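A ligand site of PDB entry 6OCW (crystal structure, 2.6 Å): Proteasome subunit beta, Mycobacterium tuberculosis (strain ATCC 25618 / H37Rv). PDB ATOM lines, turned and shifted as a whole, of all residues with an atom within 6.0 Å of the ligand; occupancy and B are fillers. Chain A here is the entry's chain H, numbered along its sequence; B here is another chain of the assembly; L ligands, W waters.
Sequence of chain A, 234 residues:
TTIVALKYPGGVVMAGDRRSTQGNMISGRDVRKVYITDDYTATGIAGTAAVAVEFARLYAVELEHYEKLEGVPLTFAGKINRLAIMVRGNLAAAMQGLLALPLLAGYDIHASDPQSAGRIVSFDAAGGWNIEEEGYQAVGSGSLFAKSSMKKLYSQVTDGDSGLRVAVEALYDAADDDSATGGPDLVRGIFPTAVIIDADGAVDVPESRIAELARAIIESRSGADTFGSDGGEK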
ATOM      1  N   THR A   1      -3.819 -20.744 -12.310  1.00  0.00           N
ATOM      2  CA  THR A   1      -3.194 -19.558 -12.906  1.00  0.00           C
ATOM      3  C   THR A   1      -1.686 -19.566 -12.693  1.00  0.00           C
ATOM      4  O   THR A   1      -1.219 -19.987 -11.635  1.00  0.00           O
ATOM      5  CB  THR A   1      -3.776 -18.234 -12.322  1.00  0.00           C
ATOM      6  OG1 THR A   1      -5.078 -17.973 -12.858  1.00  0.00           O
ATOM      7  CG2 THR A   1      -2.829 -17.042 -12.610  1.00  0.00           C
ATOM      8  N   ARG A  19      -6.402 -19.759 -18.512  1.00  0.00           N
ATOM      9  CA  ARG A  19      -7.322 -20.779 -18.040  1.00  0.00           C
ATOM     10  C   ARG A  19      -8.184 -20.290 -16.886  1.00  0.00           C
ATOM     11  O   ARG A  19      -7.715 -19.570 -16.005  1.00  0.00           O
ATOM     12  CB  ARG A  19      -6.579 -22.034 -17.611  1.00  0.00           C
ATOM     13  CG  ARG A  19      -7.488 -23.050 -16.971  1.00  0.00           C
ATOM     14  CD  ARG A  19      -6.870 -24.410 -16.982  1.00  0.00           C
ATOM     15  NE  ARG A  19      -6.914 -24.996 -18.318  1.00  0.00           N
ATOM     16  CZ  ARG A  19      -6.425 -26.197 -18.599  1.00  0.00           C
ATOM     17  NH1 ARG A  19      -5.880 -26.936 -17.640  1.00  0.00           N
ATOM     18  NH2 ARG A  19      -6.504 -26.671 -19.822  1.00  0.00           N
ATOM     19  N   SER A  20      -9.437 -20.717 -16.894  1.00  0.00           N
ATOM     20  CA  SER A  20     -10.350 -20.472 -15.789  1.00  0.00           C
ATOM     21  C   SER A  20     -10.979 -21.816 -15.392  1.00  0.00           C
ATOM     22  O   SER A  20     -11.441 -22.560 -16.257  1.00  0.00           O
ATOM     23  CB  SER A  20     -11.401 -19.452 -16.203  1.00  0.00           C
ATOM     24  OG  SER A  20     -12.583 -19.616 -15.465  1.00  0.00           O
ATOM     25  N   THR A  21     -10.978 -22.118 -14.086  1.00  0.00           N
ATOM     26  CA  THR A  21     -11.536 -23.360 -13.566  1.00  0.00           C
ATOM     27  C   THR A  21     -12.557 -23.090 -12.479  1.00  0.00           C
ATOM     28  O   THR A  21     -12.524 -22.072 -11.793  1.00  0.00           O
ATOM     29  CB  THR A  21     -10.472 -24.291 -12.967  1.00  0.00           C
ATOM     30  OG1 THR A  21      -9.660 -23.555 -12.040  1.00  0.00           O
ATOM     31  CG2 THR A  21      -9.618 -24.925 -14.059  1.00  0.00           C
ATOM     32  N   GLN A  22     -13.461 -24.056 -12.313  1.00  0.00           N
ATOM     33  CA  GLN A  22     -14.289 -24.198 -11.105  1.00  0.00           C
ATOM     34  C   GLN A  22     -14.090 -25.636 -10.648  1.00  0.00           C
ATOM     35  O   GLN A  22     -14.627 -26.574 -11.244  1.00  0.00           O
ATOM     36  CB  GLN A  22     -15.757 -23.890 -11.373  1.00  0.00           C
ATOM     37  CG  GLN A  22     -16.002 -22.427 -11.583  1.00  0.00           C
ATOM     38  CD  GLN A  22     -17.460 -22.062 -11.765  1.00  0.00           C
ATOM     39  OE1 GLN A  22     -18.351 -22.676 -11.161  1.00  0.00           O
ATOM     40  NE2 GLN A  22     -17.711 -21.047 -12.587  1.00  0.00           N
ATOM     41  N   SER A  27     -13.621 -23.827 -17.114  1.00  0.00           N
ATOM     42  CA  SER A  27     -14.702 -22.889 -17.353  1.00  0.00           C
ATOM     43  C   SER A  27     -14.312 -21.759 -18.268  1.00  0.00           C
ATOM     44  O   SER A  27     -15.194 -21.010 -18.699  1.00  0.00           O
ATOM     45  CB  SER A  27     -15.203 -22.303 -16.032  1.00  0.00           C
ATOM     46  OG  SER A  27     -14.170 -21.610 -15.356  1.00  0.00           O
ATOM     47  N   GLY A  28     -13.022 -21.596 -18.560  1.00  0.00           N
ATOM     48  CA  GLY A  28     -12.582 -20.581 -19.483  1.00  0.00           C
ATOM     49  C   GLY A  28     -11.262 -20.947 -20.132  1.00  0.00           C
ATOM     50  O   GLY A  28     -10.407 -21.547 -19.477  1.00  0.00           O
ATOM     51  N   VAL A  31      -9.330 -16.370 -20.995  1.00  0.00           N
ATOM     52  CA  VAL A  31      -9.367 -15.296 -20.017  1.00  0.00           C
ATOM     53  C   VAL A  31      -8.051 -14.536 -20.105  1.00  0.00           C
ATOM     54  O   VAL A  31      -7.008 -15.080 -20.486  1.00  0.00           O
ATOM     55  CB  VAL A  31      -9.616 -15.829 -18.596  1.00  0.00           C
ATOM     56  CG1 VAL A  31     -10.905 -16.630 -18.575  1.00  0.00           C
ATOM     57  CG2 VAL A  31      -8.468 -16.692 -18.136  1.00  0.00           C
ATOM     58  N   ARG A  32      -8.121 -13.254 -19.797  1.00  0.00           N
ATOM     59  CA  ARG A  32      -6.960 -12.373 -19.796  1.00  0.00           C
ATOM     60  C   ARG A  32      -6.623 -12.053 -18.347  1.00  0.00           C
ATOM     61  O   ARG A  32      -7.486 -11.608 -17.595  1.00  0.00           O
ATOM     62  CB  ARG A  32      -7.250 -11.100 -20.588  1.00  0.00           C
ATOM     63  CG  ARG A  32      -6.039 -10.210 -20.785  1.00  0.00           C
ATOM     64  CD  ARG A  32      -6.299  -9.177 -21.852  1.00  0.00           C
ATOM     65  NE  ARG A  32      -5.070  -8.495 -22.266  1.00  0.00           N
ATOM     66  CZ  ARG A  32      -4.928  -7.902 -23.440  1.00  0.00           C
ATOM     67  NH1 ARG A  32      -5.938  -7.900 -24.304  1.00  0.00           N
ATOM     68  NH2 ARG A  32      -3.791  -7.296 -23.758  1.00  0.00           N
ATOM     69  N   LYS A  33      -5.371 -12.319 -17.963  1.00  0.00           N
ATOM     70  CA  LYS A  33      -4.949 -12.097 -16.587  1.00  0.00           C
ATOM     71  C   LYS A  33      -3.855 -11.050 -16.445  1.00  0.00           C
ATOM     72  O   LYS A  33      -3.514 -10.690 -15.306  1.00  0.00           O
ATOM     73  CB  LYS A  33      -4.462 -13.403 -15.932  1.00  0.00           C
ATOM     74  CG  LYS A  33      -5.452 -14.548 -16.021  1.00  0.00           C
ATOM     75  CD  LYS A  33      -4.827 -15.844 -15.543  1.00  0.00           C
ATOM     76  CE  LYS A  33      -5.805 -16.989 -15.661  1.00  0.00           C
ATOM     77  NZ  LYS A  33      -5.173 -18.284 -15.326  1.00  0.00           N
ATOM     78  N   TYR A  35      -2.679  -7.157 -17.577  1.00  0.00           N
ATOM     79  CA  TYR A  35      -3.218  -5.910 -18.117  1.00  0.00           C
ATOM     80  C   TYR A  35      -2.202  -4.779 -18.049  1.00  0.00           C
ATOM     81  O   TYR A  35      -1.392  -4.700 -17.109  1.00  0.00           O
ATOM     82  CB  TYR A  35      -4.481  -5.475 -17.375  1.00  0.00           C
ATOM     83  CG  TYR A  35      -5.635  -6.433 -17.566  1.00  0.00           C
ATOM     84  CD1 TYR A  35      -6.467  -6.334 -18.687  1.00  0.00           C
ATOM     85  CD2 TYR A  35      -5.907  -7.428 -16.628  1.00  0.00           C
ATOM     86  CE1 TYR A  35      -7.531  -7.209 -18.871  1.00  0.00           C
ATOM     87  CE2 TYR A  35      -6.971  -8.304 -16.802  1.00  0.00           C
ATOM     88  CZ  TYR A  35      -7.778  -8.188 -17.916  1.00  0.00           C
ATOM     89  OH  TYR A  35      -8.838  -9.059 -18.078  1.00  0.00           O
ATOM     90  N   ILE A  45      -2.716 -10.653 -12.173  1.00  0.00           N
ATOM     91  CA  ILE A  45      -3.448 -10.966 -10.959  1.00  0.00           C
ATOM     92  C   ILE A  45      -3.967 -12.404 -11.002  1.00  0.00           C
ATOM     93  O   ILE A  45      -4.623 -12.789 -11.978  1.00  0.00           O
ATOM     94  CB  ILE A  45      -4.614 -10.001 -10.730  1.00  0.00           C
ATOM     95  CG1 ILE A  45      -4.143  -8.561 -10.950  1.00  0.00           C
ATOM     96  CG2 ILE A  45      -5.164 -10.204  -9.316  1.00  0.00           C
ATOM     97  CD1 ILE A  45      -5.207  -7.517 -10.650  1.00  0.00           C
ATOM     98  N   ALA A  46      -3.725 -13.150  -9.927  1.00  0.00           N
ATOM     99  CA  ALA A  46      -4.202 -14.515  -9.722  1.00  0.00           C
ATOM    100  C   ALA A  46      -5.291 -14.528  -8.653  1.00  0.00           C
ATOM    101  O   ALA A  46      -5.332 -13.666  -7.782  1.00  0.00           O
ATOM    102  CB  ALA A  46      -3.061 -15.434  -9.317  1.00  0.00           C
ATOM    103  N   GLY A  47      -6.165 -15.526  -8.706  1.00  0.00           N
ATOM    104  CA  GLY A  47      -7.224 -15.627  -7.724  1.00  0.00           C
ATOM    105  C   GLY A  47      -8.594 -15.808  -8.352  1.00  0.00           C
ATOM    106  O   GLY A  47      -8.725 -16.443  -9.390  1.00  0.00           O
ATOM    107  N   THR A  48      -9.624 -15.247  -7.718  1.00  0.00           N
ATOM    108  CA  THR A  48     -10.974 -15.277  -8.250  1.00  0.00           C
ATOM    109  C   THR A  48     -11.088 -14.342  -9.454  1.00  0.00           C
ATOM    110  O   THR A  48     -10.844 -13.135  -9.320  1.00  0.00           O
ATOM    111  CB  THR A  48     -11.952 -14.870  -7.170  1.00  0.00           C
ATOM    112  OG1 THR A  48     -11.567 -15.489  -5.937  1.00  0.00           O
ATOM    113  CG2 THR A  48     -13.378 -15.287  -7.526  1.00  0.00           C
ATOM    114  N   ALA A  49     -11.508 -14.886 -10.601  1.00  0.00           N
ATOM    115  CA  ALA A  49     -11.502 -14.136 -11.850  1.00  0.00           C
ATOM    116  C   ALA A  49     -12.176 -12.775 -11.702  1.00  0.00           C
ATOM    117  O   ALA A  49     -11.654 -11.747 -12.159  1.00  0.00           O
ATOM    118  CB  ALA A  49     -12.179 -14.966 -12.945  1.00  0.00           C
ATOM    119  N   ALA A  50     -13.355 -12.749 -11.078  1.00  0.00           N
ATOM    120  CA  ALA A  50     -14.124 -11.507 -10.977  1.00  0.00           C
ATOM    121  C   ALA A  50     -13.363 -10.471 -10.168  1.00  0.00           C
ATOM    122  O   ALA A  50     -13.324  -9.287 -10.537  1.00  0.00           O
ATOM    123  CB  ALA A  50     -15.478 -11.790 -10.348  1.00  0.00           C
ATOM    124  N   ALA A  52     -10.046 -10.385  -9.569  1.00  0.00           N
ATOM    125  CA  ALA A  52      -8.789 -10.000 -10.198  1.00  0.00           C
ATOM    126  C   ALA A  52      -9.041  -8.957 -11.272  1.00  0.00           C
ATOM    127  O   ALA A  52      -8.338  -7.928 -11.347  1.00  0.00           O
ATOM    128  CB  ALA A  52      -8.074 -11.218 -10.785  1.00  0.00           C
ATOM    129  N   VAL A  53     -10.042  -9.206 -12.107  1.00  0.00           N
ATOM    130  CA  VAL A  53     -10.370  -8.246 -13.146  1.00  0.00           C
ATOM    131  C   VAL A  53     -10.799  -6.921 -12.533  1.00  0.00           C
ATOM    132  O   VAL A  53     -10.312  -5.859 -12.925  1.00  0.00           O
ATOM    133  CB  VAL A  53     -11.432  -8.830 -14.101  1.00  0.00           C
ATOM    134  CG1 VAL A  53     -11.862  -7.775 -15.102  1.00  0.00           C
ATOM    135  CG2 VAL A  53     -10.846 -10.026 -14.812  1.00  0.00           C
ATOM    136  N   GLY A  97     -12.847 -16.343   0.388  1.00  0.00           N
ATOM    137  CA  GLY A  97     -12.834 -16.920  -0.950  1.00  0.00           C
ATOM    138  C   GLY A  97     -12.806 -15.935  -2.126  1.00  0.00           C
ATOM    139  O   GLY A  97     -12.821 -16.379  -3.273  1.00  0.00           O
ATOM    140  N   LEU A  98     -12.771 -14.627  -1.872  1.00  0.00           N
ATOM    141  CA  LEU A  98     -12.657 -13.649  -2.946  1.00  0.00           C
ATOM    142  C   LEU A  98     -11.216 -13.139  -3.011  1.00  0.00           C
ATOM    143  O   LEU A  98     -10.899 -12.014  -2.627  1.00  0.00           O
ATOM    144  CB  LEU A  98     -13.652 -12.527  -2.733  1.00  0.00           C
ATOM    145  CG  LEU A  98     -15.062 -13.098  -2.637  1.00  0.00           C
ATOM    146  CD1 LEU A  98     -16.074 -11.999  -2.390  1.00  0.00           C
ATOM    147  CD2 LEU A  98     -15.384 -13.867  -3.902  1.00  0.00           C
ATOM    148  N   ALA A 180      -4.444 -26.194 -13.000  1.00  0.00           N
ATOM    149  CA  ALA A 180      -5.210 -24.956 -13.065  1.00  0.00           C
ATOM    150  C   ALA A 180      -4.535 -23.917 -13.944  1.00  0.00           C
ATOM    151  O   ALA A 180      -5.055 -22.799 -14.076  1.00  0.00           O
ATOM    152  CB  ALA A 180      -5.434 -24.393 -11.653  1.00  0.00           C
ATOM    153  N   LEU B  91     -24.275 -11.807  -4.462  1.00  0.00           N
ATOM    154  CA  LEU B  91     -23.485 -12.969  -4.028  1.00  0.00           C
ATOM    155  C   LEU B  91     -23.881 -13.496  -2.634  1.00  0.00           C
ATOM    156  O   LEU B  91     -24.014 -14.710  -2.437  1.00  0.00           O
ATOM    157  CB  LEU B  91     -21.992 -12.639  -4.063  1.00  0.00           C
ATOM    158  CG  LEU B  91     -21.034 -13.722  -3.509  1.00  0.00           C
ATOM    159  CD1 LEU B  91     -21.193 -15.032  -4.243  1.00  0.00           C
ATOM    160  CD2 LEU B  91     -19.586 -13.268  -3.575  1.00  0.00           C
ATOM    161  N   MET B  95     -25.307 -17.204  -1.801  1.00  0.00           N
ATOM    162  CA  MET B  95     -24.750 -18.219  -0.911  1.00  0.00           C
ATOM    163  C   MET B  95     -25.772 -18.698   0.097  1.00  0.00           C
ATOM    164  O   MET B  95     -25.667 -19.833   0.577  1.00  0.00           O
ATOM    165  CB  MET B  95     -23.530 -17.680  -0.173  1.00  0.00           C
ATOM    166  CG  MET B  95     -22.293 -17.520  -1.038  1.00  0.00           C
ATOM    167  SD  MET B  95     -21.032 -16.679  -0.065  1.00  0.00           S
ATOM    168  CE  MET B  95     -21.837 -15.107   0.287  1.00  0.00           C
ATOM    169  N   SER B 122     -20.976 -14.993 -20.729  1.00  0.00           N
ATOM    170  CA  SER B 122     -21.272 -15.817 -19.562  1.00  0.00           C
ATOM    171  C   SER B 122     -20.785 -15.130 -18.284  1.00  0.00           C
ATOM    172  O   SER B 122     -19.895 -14.273 -18.280  1.00  0.00           O
ATOM    173  CB  SER B 122     -20.675 -17.214 -19.697  1.00  0.00           C
ATOM    174  OG  SER B 122     -19.328 -17.197 -20.126  1.00  0.00           O
ATOM    175  N   PHE B 123     -21.428 -15.517 -17.179  1.00  0.00           N
ATOM    176  CA  PHE B 123     -21.150 -14.954 -15.860  1.00  0.00           C
ATOM    177  C   PHE B 123     -20.970 -16.086 -14.866  1.00  0.00           C
ATOM    178  O   PHE B 123     -21.458 -17.197 -15.071  1.00  0.00           O
ATOM    179  CB  PHE B 123     -22.286 -14.061 -15.395  1.00  0.00           C
ATOM    180  CG  PHE B 123     -22.504 -12.838 -16.251  1.00  0.00           C
ATOM    181  CD1 PHE B 123     -23.177 -12.921 -17.443  1.00  0.00           C
ATOM    182  CD2 PHE B 123     -22.055 -11.594 -15.826  1.00  0.00           C
ATOM    183  CE1 PHE B 123     -23.381 -11.800 -18.216  1.00  0.00           C
ATOM    184  CE2 PHE B 123     -22.280 -10.484 -16.594  1.00  0.00           C
ATOM    185  CZ  PHE B 123     -22.929 -10.586 -17.787  1.00  0.00           C
ATOM    186  N   ASP B 124     -20.285 -15.786 -13.770  1.00  0.00           N
ATOM    187  CA  ASP B 124     -20.268 -16.649 -12.594  1.00  0.00           C
ATOM    188  C   ASP B 124     -21.001 -15.962 -11.433  1.00  0.00           C
ATOM    189  O   ASP B 124     -21.469 -14.826 -11.545  1.00  0.00           O
ATOM    190  CB  ASP B 124     -18.827 -17.031 -12.232  1.00  0.00           C
ATOM    191  CG  ASP B 124     -18.004 -15.833 -11.679  1.00  0.00           C
ATOM    192  OD1 ASP B 124     -18.593 -14.839 -11.197  1.00  0.00           O
ATOM    193  OD2 ASP B 124     -16.754 -15.916 -11.709  1.00  0.00           O
ATOM    194  N   ALA B 125     -21.074 -16.661 -10.305  1.00  0.00           N
ATOM    195  CA  ALA B 125     -21.798 -16.124  -9.145  1.00  0.00           C
ATOM    196  C   ALA B 125     -21.114 -14.914  -8.534  1.00  0.00           C
ATOM    197  O   ALA B 125     -21.744 -14.186  -7.764  1.00  0.00           O
ATOM    198  CB  ALA B 125     -21.978 -17.204  -8.080  1.00  0.00           C
ATOM    199  N   ALA B 126     -19.831 -14.694  -8.824  1.00  0.00           N
ATOM    200  CA  ALA B 126     -19.113 -13.570  -8.228  1.00  0.00           C
ATOM    201  C   ALA B 126     -19.195 -12.303  -9.068  1.00  0.00           C
ATOM    202  O   ALA B 126     -18.687 -11.261  -8.648  1.00  0.00           O
ATOM    203  CB  ALA B 126     -17.642 -13.939  -7.983  1.00  0.00           C
ATOM    204  N   GLY B 128     -17.937 -12.247 -12.219  1.00  0.00           N
ATOM    205  CA  GLY B 128     -17.030 -12.417 -13.340  1.00  0.00           C
ATOM    206  C   GLY B 128     -17.780 -12.725 -14.620  1.00  0.00           C
ATOM    207  O   GLY B 128     -18.858 -13.336 -14.605  1.00  0.00           O
ATOM    208  N   TRP B 129     -17.219 -12.280 -15.744  1.00  0.00           N
ATOM    209  CA  TRP B 129     -17.846 -12.528 -17.027  1.00  0.00           C
ATOM    210  C   TRP B 129     -16.772 -12.829 -18.063  1.00  0.00           C
ATOM    211  O   TRP B 129     -15.586 -12.567 -17.862  1.00  0.00           O
ATOM    212  CB  TRP B 129     -18.716 -11.353 -17.468  1.00  0.00           C
ATOM    213  CG  TRP B 129     -18.049 -10.035 -17.413  1.00  0.00           C
ATOM    214  CD1 TRP B 129     -18.044  -9.155 -16.379  1.00  0.00           C
ATOM    215  CD2 TRP B 129     -17.304  -9.404 -18.464  1.00  0.00           C
ATOM    216  NE1 TRP B 129     -17.323  -8.023 -16.707  1.00  0.00           N
ATOM    217  CE2 TRP B 129     -16.858  -8.152 -17.976  1.00  0.00           C
ATOM    218  CE3 TRP B 129     -16.956  -9.796 -19.772  1.00  0.00           C
ATOM    219  CZ2 TRP B 129     -16.101  -7.277 -18.746  1.00  0.00           C
ATOM    220  CZ3 TRP B 129     -16.194  -8.915 -20.531  1.00  0.00           C
ATOM    221  CH2 TRP B 129     -15.772  -7.678 -20.018  1.00  0.00           C
ATOM    222  N   ASN B 130     -17.215 -13.404 -19.178  1.00  0.00           N
ATOM    223  CA  ASN B 130     -16.332 -13.671 -20.301  1.00  0.00           C
ATOM    224  C   ASN B 130     -17.162 -13.658 -21.574  1.00  0.00           C
ATOM    225  O   ASN B 130     -18.246 -14.239 -21.636  1.00  0.00           O
ATOM    226  CB  ASN B 130     -15.615 -15.012 -20.121  1.00  0.00           C
ATOM    227  CG  ASN B 130     -14.659 -15.329 -21.267  1.00  0.00           C
ATOM    228  OD1 ASN B 130     -15.043 -15.967 -22.244  1.00  0.00           O
ATOM    229  ND2 ASN B 130     -13.410 -14.899 -21.135  1.00  0.00           N
HETATM  230  C1  LIG L   1     -16.754 -18.293  -7.306  1.00  0.00           C
HETATM  231  C2  LIG L   1     -18.028 -17.882  -6.961  1.00  0.00           C
HETATM  232  C3  LIG L   1     -18.488 -17.477  -5.581  1.00  0.00           C
HETATM  233  O1  LIG L   1     -18.762 -17.917  -8.109  1.00  0.00           O
HETATM  234  N1  LIG L   1     -17.960 -18.342  -9.153  1.00  0.00           N
HETATM  235  C4  LIG L   1     -16.760 -18.583  -8.677  1.00  0.00           C
HETATM  236  C5  LIG L   1     -15.569 -19.058  -9.488  1.00  0.00           C
HETATM  237  O2  LIG L   1     -14.815 -19.855  -9.083  1.00  0.00           O
HETATM  238  C6  LIG L   1     -17.572 -16.020 -15.838  1.00  0.00           C
HETATM  239  C7  LIG L   1     -15.219 -16.548 -15.458  1.00  0.00           C
HETATM  240  C8  LIG L   1     -12.909 -18.465 -10.880  1.00  0.00           C
HETATM  241  C9  LIG L   1     -14.197 -18.949 -11.543  1.00  0.00           C
HETATM  242  C10 LIG L   1     -14.180 -18.309 -12.928  1.00  0.00           C
HETATM  243  C11 LIG L   1     -15.243 -18.843 -13.914  1.00  0.00           C
HETATM  244  C12 LIG L   1     -16.686 -18.222 -16.223  1.00  0.00           C
HETATM  245  C13 LIG L   1     -17.878 -17.274 -16.299  1.00  0.00           C
HETATM  246  C14 LIG L   1     -16.279 -15.626 -16.080  1.00  0.00           C
HETATM  247  C15 LIG L   1     -14.062 -16.701 -16.380  1.00  0.00           C
HETATM  248  N2  LIG L   1     -15.676 -17.998 -15.032  1.00  0.00           N
HETATM  249  N3  LIG L   1     -15.324 -18.468 -10.825  1.00  0.00           N
HETATM  250  O3  LIG L   1     -12.785 -17.383 -10.417  1.00  0.00           O
HETATM  251  O4  LIG L   1     -15.686 -19.915 -13.766  1.00  0.00           O
HETATM  252  N4  LIG L   1     -11.846 -19.464 -10.862  1.00  0.00           N
HETATM  253  C16 LIG L   1     -10.518 -19.217 -10.297  1.00  0.00           C
HETATM  254  C17 LIG L   1      -9.718 -18.912 -11.576  1.00  0.00           C
HETATM  255  O5  LIG L   1      -9.841 -19.623 -12.516  1.00  0.00           O
HETATM  256  C18 LIG L   1     -10.068 -20.505  -9.653  1.00  0.00           C
HETATM  257  C19 LIG L   1      -8.089 -17.511 -12.961  1.00  0.00           C
HETATM  258  C20 LIG L   1      -8.148 -15.994 -13.354  1.00  0.00           C
HETATM  259  C21 LIG L   1      -7.281 -15.136 -12.744  1.00  0.00           C
HETATM  260  C22 LIG L   1      -7.316 -13.772 -13.084  1.00  0.00           C
HETATM  261  C23 LIG L   1      -8.226 -13.324 -14.036  1.00  0.00           C
HETATM  262  C24 LIG L   1      -9.090 -14.211 -14.641  1.00  0.00           C
HETATM  263  C25 LIG L   1      -9.057 -15.546 -14.306  1.00  0.00           C
HETATM  264  F1  LIG L   1      -8.264 -11.997 -14.374  1.00  0.00           F
HETATM  265  F2  LIG L   1      -9.916 -16.410 -14.915  1.00  0.00           F
HETATM  266  N5  LIG L   1      -8.824 -17.731 -11.697  1.00  0.00           N
HETATM  267  O   HOH W   1      -7.900 -21.784 -13.217  1.00  0.00           O
HETATM  268  O   HOH W   2     -20.685 -19.505 -10.693  1.00  0.00           O
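The side-chain amide nitrogen (NE2) of Gln 22 lies within hydrogen-bond range of an oxygen (O4) of the ligand (2.6 Å). The backbone carbonyl oxygen (O) of Gly 47 lies within hydrogen-bond range of a nitrogen (N5) of the ligand (2.6 Å). The side-chain hydroxyl (OG) of Ser 27 sits at hydrogen-bond distance from an oxygen (O4) of the ligand, at 2.8 Å. O3 of the ligand is in hydrogen-bond range of N of Ala 49, 2.8 Å away. O5 of the ligand lies within hydrogen-bond range of N of Thr 21, at 3.2 Å. O of Thr 21 is in hydrogen-bond range of N4 of the ligand, 2.9 Å away. The side-chain carboxylate of Asp 124 of chain B is in hydrogen-bond range of a nitrogen (N3) of the ligand. O1 of the ligand lies close to N of Ala 125 of chain B (3.4 Å). The backbone NH (N) of Ala 126 of chain B sits at hydrogen-bond distance from an oxygen (O1) of the ligand, 3.5 Å away.
Water W1 lies within hydrogen-bond range of the side-chain hydroxyl of Thr 21 (2.8 Å), an oxygen (O5) of the ligand (3.0 Å) and the backbone carbonyl oxygen of Ala 180 (3.1 Å). Water W2 lies within hydrogen-bond range of the backbone NH (N) of Ala 125 of chain B (2.9 Å) and a nitrogen (N1) of the ligand (3.3 Å).
The side-chain hydroxyl (OG) of Ser 27 lies within hydrogen-bond range of the backbone NH (N) of Thr 21. OG of Ser 20 lies within hydrogen-bond range of OG of Ser 27 (2.6 Å). N of Thr 1 sits at hydrogen-bond distance from O of Ala 180 (3.0 Å). The side-chain carboxylate (OD1) of Asp 124 of chain B is in hydrogen-bond range of the backbone NH (N) of Gly 128 of chain B, at 2.9 Å. The backbone NH (N) of Ile 45 is in hydrogen-bond range of the backbone carbonyl oxygen (O) of Lys 33 (3.2 Å). O of Gly 28 is in hydrogen-bond range of N of Ser 20 (2.9 Å). The backbone carbonyl oxygen (O) of Arg 32 lies within hydrogen-bond range of the side-chain hydroxyl (OH) of Tyr 35. The backbone carbonyl oxygen of Ser 122 of chain B is in hydrogen-bond range of the backbone NH of Asn 130 of chain B (3.0 Å).
O of Arg 32 lies close to F1 of the ligand (3.3 Å). Merely in contact with the ligand: Thr 1, Ile 45, Ser 20, Gly 128 of chain B, Val 53, Lys 33, Trp 129 of chain B, Ala 52, Thr 48, Phe 123 of chain B, Val 31, Arg 19, Ser 122 of chain B, Leu 91 of chain B and Asn 130 of chain B. Hydrophobic or aromatic side chains within 4 Å of the ligand: Val 31, Ala 49, Ala 52, Val 53, Leu 91 of chain B and Ala 125 of chain B.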
